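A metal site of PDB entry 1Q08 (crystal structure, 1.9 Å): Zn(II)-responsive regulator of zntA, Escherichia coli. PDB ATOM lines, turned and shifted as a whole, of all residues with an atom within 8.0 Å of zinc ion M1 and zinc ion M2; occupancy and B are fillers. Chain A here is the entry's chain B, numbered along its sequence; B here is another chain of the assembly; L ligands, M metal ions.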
ATOM      1  N   LEU A  68      19.661 -24.362  15.322  1.00  0.00           N
ATOM      2  CA  LEU A  68      19.183 -23.151  15.999  1.00  0.00           C
ATOM      3  C   LEU A  68      18.600 -23.535  17.354  1.00  0.00           C
ATOM      4  O   LEU A  68      18.857 -22.888  18.368  1.00  0.00           O
ATOM      5  CB  LEU A  68      18.109 -22.456  15.161  1.00  0.00           C
ATOM      6  CG  LEU A  68      18.540 -21.773  13.860  1.00  0.00           C
ATOM      7  CD1 LEU A  68      17.317 -21.285  13.112  1.00  0.00           C
ATOM      8  CD2 LEU A  68      19.466 -20.603  14.171  1.00  0.00           C
ATOM      9  N   ASN A  69      17.802 -24.598  17.340  1.00  0.00           N
ATOM     10  CA  ASN A  69      17.168 -25.099  18.538  1.00  0.00           C
ATOM     11  C   ASN A  69      18.164 -25.501  19.627  1.00  0.00           C
ATOM     12  O   ASN A  69      18.074 -25.042  20.777  1.00  0.00           O
ATOM     13  CB  ASN A  69      16.319 -26.320  18.203  1.00  0.00           C
ATOM     14  CG  ASN A  69      15.645 -26.905  19.427  1.00  0.00           C
ATOM     15  OD1 ASN A  69      14.575 -26.454  19.836  1.00  0.00           O
ATOM     16  ND2 ASN A  69      16.283 -27.909  20.027  1.00  0.00           N
ATOM     17  N   ALA A  71      21.301 -24.730  20.221  1.00  0.00           N
ATOM     18  CA  ALA A  71      22.221 -23.746  20.797  1.00  0.00           C
ATOM     19  C   ALA A  71      21.569 -22.785  21.795  1.00  0.00           C
ATOM     20  O   ALA A  71      22.275 -22.154  22.590  1.00  0.00           O
ATOM     21  CB  ALA A  71      22.893 -22.945  19.680  1.00  0.00           C
ATOM     22  N   CYS A  72      20.247 -22.685  21.759  1.00  0.00           N
ATOM     23  CA  CYS A  72      19.527 -21.770  22.637  1.00  0.00           C
ATOM     24  C   CYS A  72      19.100 -22.409  23.952  1.00  0.00           C
ATOM     25  O   CYS A  72      18.610 -23.545  23.979  1.00  0.00           O
ATOM     26  CB  CYS A  72      18.300 -21.222  21.890  1.00  0.00           C
ATOM     27  SG  CYS A  72      17.287 -20.072  22.840  1.00  0.00           S
ATOM     28  N   CYS A  73      19.286 -21.681  25.060  1.00  0.00           N
ATOM     29  CA  CYS A  73      18.913 -22.196  26.376  1.00  0.00           C
ATOM     30  C   CYS A  73      17.398 -22.316  26.534  1.00  0.00           C
ATOM     31  O   CYS A  73      16.914 -23.127  27.337  1.00  0.00           O
ATOM     32  CB  CYS A  73      19.451 -21.283  27.483  1.00  0.00           C
ATOM     33  SG  CYS A  73      18.519 -19.740  27.724  1.00  0.00           S
ATOM     34  N   GLY A  74      16.666 -21.512  25.776  1.00  0.00           N
ATOM     35  CA  GLY A  74      15.213 -21.550  25.827  1.00  0.00           C
ATOM     36  C   GLY A  74      14.570 -21.137  27.153  1.00  0.00           C
ATOM     37  O   GLY A  74      13.457 -21.571  27.455  1.00  0.00           O
ATOM     38  N   THR A  75      15.254 -20.303  27.929  1.00  0.00           N
ATOM     39  CA  THR A  75      14.717 -19.868  29.220  1.00  0.00           C
ATOM     40  C   THR A  75      14.461 -18.364  29.277  1.00  0.00           C
ATOM     41  O   THR A  75      14.475 -17.685  28.249  1.00  0.00           O
ATOM     42  CB  THR A  75      15.671 -20.257  30.371  1.00  0.00           C
ATOM     43  OG1 THR A  75      16.877 -19.489  30.270  1.00  0.00           O
ATOM     44  CG2 THR A  75      16.033 -21.739  30.279  1.00  0.00           C
ATOM     45  N   ALA A  76      14.215 -17.848  30.475  1.00  0.00           N
ATOM     46  CA  ALA A  76      13.956 -16.418  30.669  1.00  0.00           C
ATOM     47  C   ALA A  76      15.129 -15.543  30.238  1.00  0.00           C
ATOM     48  O   ALA A  76      15.012 -14.315  30.164  1.00  0.00           O
ATOM     49  CB  ALA A  76      13.603 -16.150  32.130  1.00  0.00           C
ATOM     50  N   HIS A  77      16.271 -16.177  29.969  1.00  0.00           N
ATOM     51  CA  HIS A  77      17.492 -15.498  29.511  1.00  0.00           C
ATOM     52  C   HIS A  77      17.088 -14.409  28.512  1.00  0.00           C
ATOM     53  O   HIS A  77      16.375 -14.685  27.553  1.00  0.00           O
ATOM     54  CB  HIS A  77      18.401 -16.531  28.823  1.00  0.00           C
ATOM     55  CG  HIS A  77      19.823 -16.087  28.640  1.00  0.00           C
ATOM     56  ND1 HIS A  77      20.626 -16.604  27.651  1.00  0.00           N
ATOM     57  CD2 HIS A  77      20.589 -15.226  29.342  1.00  0.00           C
ATOM     58  CE1 HIS A  77      21.833 -16.072  27.743  1.00  0.00           C
ATOM     59  NE2 HIS A  77      21.831 -15.231  28.768  1.00  0.00           N
ATOM     60  N   SER A  78      17.558 -13.186  28.729  1.00  0.00           N
ATOM     61  CA  SER A  78      17.218 -12.066  27.836  1.00  0.00           C
ATOM     62  C   SER A  78      17.635 -12.336  26.396  1.00  0.00           C
ATOM     63  O   SER A  78      18.762 -12.753  26.122  1.00  0.00           O
ATOM     64  CB  SER A  78      17.885 -10.777  28.322  1.00  0.00           C
ATOM     65  OG  SER A  78      17.642  -9.718  27.424  1.00  0.00           O
ATOM     66  N   SER A  79      16.715 -12.073  25.462  1.00  0.00           N
ATOM     67  CA  SER A  79      16.998 -12.313  24.045  1.00  0.00           C
ATOM     68  C   SER A  79      18.129 -11.438  23.526  1.00  0.00           C
ATOM     69  O   SER A  79      18.546 -11.566  22.371  1.00  0.00           O
ATOM     70  CB  SER A  79      15.736 -12.118  23.196  1.00  0.00           C
ATOM     71  OG  SER A  79      15.313 -10.777  23.189  1.00  0.00           O
ATOM     72  N   VAL A  80      18.631 -10.532  24.360  1.00  0.00           N
ATOM     73  CA  VAL A  80      19.747  -9.685  23.950  1.00  0.00           C
ATOM     74  C   VAL A  80      20.935 -10.595  23.648  1.00  0.00           C
ATOM     75  O   VAL A  80      21.784 -10.278  22.816  1.00  0.00           O
ATOM     76  CB  VAL A  80      20.150  -8.706  25.089  1.00  0.00           C
ATOM     77  CG1 VAL A  80      21.537  -8.117  24.817  1.00  0.00           C
ATOM     78  CG2 VAL A  80      19.119  -7.595  25.214  1.00  0.00           C
ATOM     79  N   TYR A  81      20.956 -11.749  24.303  1.00  0.00           N
ATOM     80  CA  TYR A  81      22.042 -12.716  24.142  1.00  0.00           C
ATOM     81  C   TYR A  81      21.673 -13.942  23.313  1.00  0.00           C
ATOM     82  O   TYR A  81      22.485 -14.857  23.179  1.00  0.00           O
ATOM     83  CB  TYR A  81      22.517 -13.204  25.509  1.00  0.00           C
ATOM     84  CG  TYR A  81      22.759 -12.107  26.518  1.00  0.00           C
ATOM     85  CD1 TYR A  81      21.823 -11.810  27.502  1.00  0.00           C
ATOM     86  CD2 TYR A  81      23.938 -11.358  26.492  1.00  0.00           C
ATOM     87  CE1 TYR A  81      22.045 -10.791  28.435  1.00  0.00           C
ATOM     88  CE2 TYR A  81      24.177 -10.344  27.408  1.00  0.00           C
ATOM     89  CZ  TYR A  81      23.223 -10.072  28.381  1.00  0.00           C
ATOM     90  OH  TYR A  81      23.468  -9.074  29.296  1.00  0.00           O
ATOM     91  N   CYS A  82      20.471 -13.965  22.749  1.00  0.00           N
ATOM     92  CA  CYS A  82      20.042 -15.136  21.992  1.00  0.00           C
ATOM     93  C   CYS A  82      20.817 -15.480  20.736  1.00  0.00           C
ATOM     94  O   CYS A  82      20.978 -14.661  19.831  1.00  0.00           O
ATOM     95  CB  CYS A  82      18.557 -15.033  21.648  1.00  0.00           C
ATOM     96  SG  CYS A  82      17.926 -16.593  21.023  1.00  0.00           S
ATOM     97  N   SER A  83      21.265 -16.735  20.675  1.00  0.00           N
ATOM     98  CA  SER A  83      22.040 -17.257  19.555  1.00  0.00           C
ATOM     99  C   SER A  83      21.186 -17.411  18.292  1.00  0.00           C
ATOM    100  O   SER A  83      21.714 -17.420  17.180  1.00  0.00           O
ATOM    101  CB  SER A  83      22.628 -18.614  19.926  1.00  0.00           C
ATOM    102  OG  SER A  83      21.600 -19.508  20.304  1.00  0.00           O
ATOM    103  N   ILE A  84      19.875 -17.562  18.476  1.00  0.00           N
ATOM    104  CA  ILE A  84      18.967 -17.705  17.341  1.00  0.00           C
ATOM    105  C   ILE A  84      18.974 -16.410  16.519  1.00  0.00           C
ATOM    106  O   ILE A  84      19.106 -16.444  15.292  1.00  0.00           O
ATOM    107  CB  ILE A  84      17.527 -18.003  17.812  1.00  0.00           C
ATOM    108  CG1 ILE A  84      17.471 -19.377  18.498  1.00  0.00           C
ATOM    109  CG2 ILE A  84      16.557 -17.963  16.621  1.00  0.00           C
ATOM    110  CD1 ILE A  84      16.122 -19.716  19.121  1.00  0.00           C
ATOM    111  N   LEU A  85      18.831 -15.280  17.205  1.00  0.00           N
ATOM    112  CA  LEU A  85      18.835 -13.987  16.532  1.00  0.00           C
ATOM    113  C   LEU A  85      20.177 -13.729  15.860  1.00  0.00           C
ATOM    114  O   LEU A  85      20.246 -13.200  14.754  1.00  0.00           O
ATOM    115  CB  LEU A  85      18.530 -12.869  17.544  1.00  0.00           C
ATOM    116  CG  LEU A  85      17.095 -12.829  18.085  1.00  0.00           C
ATOM    117  CD1 LEU A  85      17.022 -11.848  19.246  1.00  0.00           C
ATOM    118  CD2 LEU A  85      16.137 -12.394  16.977  1.00  0.00           C
ATOM    119  N   GLU A  86      21.264 -14.110  16.539  1.00  0.00           N
ATOM    120  CA  GLU A  86      22.601 -13.927  15.989  1.00  0.00           C
ATOM    121  C   GLU A  86      22.746 -14.734  14.697  1.00  0.00           C
ATOM    122  O   GLU A  86      23.249 -14.228  13.693  1.00  0.00           O
ATOM    123  CB  GLU A  86      23.671 -14.395  16.983  1.00  0.00           C
ATOM    124  CG  GLU A  86      23.637 -13.660  18.318  1.00  0.00           C
ATOM    125  CD  GLU A  86      24.746 -14.112  19.251  1.00  0.00           C
ATOM    126  OE1 GLU A  86      24.929 -15.333  19.422  1.00  0.00           O
ATOM    127  OE2 GLU A  86      25.427 -13.240  19.828  1.00  0.00           O
ATOM    128  N   THR B  36      12.719 -12.960  25.515  1.00  0.00           N
ATOM    129  CA  THR B  36      13.600 -13.988  26.028  1.00  0.00           C
ATOM    130  C   THR B  36      13.915 -15.129  25.065  1.00  0.00           C
ATOM    131  O   THR B  36      13.303 -15.252  24.000  1.00  0.00           O
ATOM    132  CB  THR B  36      12.988 -14.632  27.287  1.00  0.00           C
ATOM    133  OG1 THR B  36      11.855 -15.407  26.894  1.00  0.00           O
ATOM    134  CG2 THR B  36      12.552 -13.560  28.265  1.00  0.00           C
ATOM    135  N   CYS B  37      14.876 -15.963  25.453  1.00  0.00           N
ATOM    136  CA  CYS B  37      15.273 -17.105  24.651  1.00  0.00           C
ATOM    137  C   CYS B  37      14.123 -18.092  24.581  1.00  0.00           C
ATOM    138  O   CYS B  37      14.006 -18.862  23.620  1.00  0.00           O
ATOM    139  CB  CYS B  37      16.501 -17.783  25.263  1.00  0.00           C
ATOM    140  SG  CYS B  37      18.025 -16.894  24.945  1.00  0.00           S
ATOM    141  N   GLN B  38      13.277 -18.096  25.597  1.00  0.00           N
ATOM    142  CA  GLN B  38      12.147 -19.005  25.603  1.00  0.00           C
ATOM    143  C   GLN B  38      11.207 -18.671  24.443  1.00  0.00           C
ATOM    144  O   GLN B  38      10.666 -19.575  23.799  1.00  0.00           O
ATOM    145  CB  GLN B  38      11.385 -18.918  26.937  1.00  0.00           C
ATOM    146  CG  GLN B  38      10.221 -19.887  27.046  1.00  0.00           C
ATOM    147  CD  GLN B  38       9.657 -19.989  28.449  1.00  0.00           C
ATOM    148  OE1 GLN B  38       8.713 -20.741  28.695  1.00  0.00           O
ATOM    149  NE2 GLN B  38      10.234 -19.239  29.381  1.00  0.00           N
ATOM    150  N   GLU B  39      11.030 -17.382  24.171  1.00  0.00           N
ATOM    151  CA  GLU B  39      10.162 -16.941  23.094  1.00  0.00           C
ATOM    152  C   GLU B  39      10.752 -17.261  21.725  1.00  0.00           C
ATOM    153  O   GLU B  39      10.063 -17.796  20.857  1.00  0.00           O
ATOM    154  CB  GLU B  39       9.901 -15.434  23.195  1.00  0.00           C
ATOM    155  CG  GLU B  39       9.283 -14.998  24.504  1.00  0.00           C
ATOM    156  CD  GLU B  39       9.160 -13.484  24.602  1.00  0.00           C
ATOM    157  OE1 GLU B  39       8.227 -12.914  23.996  1.00  0.00           O
ATOM    158  OE2 GLU B  39      10.012 -12.867  25.265  1.00  0.00           O
ATOM    159  N   SER B  40      12.027 -16.931  21.539  1.00  0.00           N
ATOM    160  CA  SER B  40      12.673 -17.198  20.255  1.00  0.00           C
ATOM    161  C   SER B  40      12.803 -18.697  20.007  1.00  0.00           C
ATOM    162  O   SER B  40      12.548 -19.173  18.892  1.00  0.00           O
ATOM    163  CB  SER B  40      14.066 -16.543  20.225  1.00  0.00           C
ATOM    164  OG  SER B  40      14.865 -16.973  21.302  1.00  0.00           O
ATOM    165  N   LYS B  41      13.162 -19.459  21.032  1.00  0.00           N
ATOM    166  CA  LYS B  41      13.295 -20.899  20.854  1.00  0.00           C
ATOM    167  C   LYS B  41      11.938 -21.538  20.546  1.00  0.00           C
ATOM    168  O   LYS B  41      11.850 -22.478  19.760  1.00  0.00           O
ATOM    169  CB  LYS B  41      13.910 -21.546  22.091  1.00  0.00           C
ATOM    170  CG  LYS B  41      14.195 -23.033  21.901  1.00  0.00           C
ATOM    171  CD  LYS B  41      15.146 -23.585  22.953  1.00  0.00           C
ATOM    172  CE  LYS B  41      15.459 -25.046  22.668  1.00  0.00           C
ATOM    173  NZ  LYS B  41      16.583 -25.586  23.491  1.00  0.00           N
HETATM  174  P1  LIG L   1      21.477 -18.387  24.058  1.00  0.00           P
HETATM  175  O1  LIG L   1      21.529 -16.986  24.555  1.00  0.00           O
HETATM  176  O2  LIG L   1      20.899 -19.267  25.099  1.00  0.00           O
HETATM  177  O3  LIG L   1      20.644 -18.443  22.835  1.00  0.00           O
HETATM  178  O4  LIG L   1      22.846 -18.849  23.733  1.00  0.00           O
HETATM  179 ZN    ZN M   1      18.526 -18.092  22.904  1.00  0.00          ZN
HETATM  180 ZN    ZN M   2      19.552 -18.143  26.354  1.00  0.00          ZN
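O3 of the ligand binds zinc ion M1, 2.1 Å away.
The side-chain sulfur (SG) of Cys 72 is bound to zinc ion M1 (2.3 Å).
Zinc ion M1 is bound by SG of Cys 37 of chain B, at 2.4 Å.
Zinc ion M1 is bound by the side-chain sulfur (SG) of Cys 82.
Three residues have an atom within 4 Å of zinc ion M2: Cys 73, His 77 and Cys 37 of chain B.
Along chain A the residues within 4 Å of zinc ion M2 span positions 73 to 77.
Merely in contact with zinc ion M1: Ser 83.
Four residues have an atom within 4 Å of zinc ion M1: Cys 72, Cys 82, Ser 83 and Cys 37 of chain B.
The nearest printed residue that does not touch zinc ion M1 is Ser 40 of chain B (4.1 Å).
OG1 of Thr 75 sits close to N of His 77.
SG of Cys 72 lies close to N of Gly 74, at 3.3 Å.
The side-chain amino group of Lys 41 of chain B is in hydrogen-bond range of the backbone carbonyl oxygen of Cys 72 (2.9 Å).
The side-chain sulfur (SG) of Cys 73 sits close to the side-chain hydroxyl (OG1) of Thr 75 (3.0 Å).
The backbone carbonyl oxygen of Cys 37 of chain B is in hydrogen-bond range of the side-chain hydroxyl of Ser 40 of chain B.
The backbone carbonyl oxygen (O) of Thr 75 lies within hydrogen-bond range of the backbone NH (N) of Cys 37 of chain B (3.3 Å).
SG of Cys 82 sits close to OG of Ser 40 of chain B, 3.1 Å away.
SG of Cys 82 lies close to N of Ile 84, 3.4 Å away.
O2 of the ligand is bound to zinc ion M2 (2.2 Å).
Zinc ion M2 is bound by ND1 of His 77 (2.3 Å).
Zinc ion M2 is bound by SG of Cys 73 (2.3 Å).
Zinc ion M2 is bound by the side-chain sulfur (SG) of Cys 37 of chain B.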
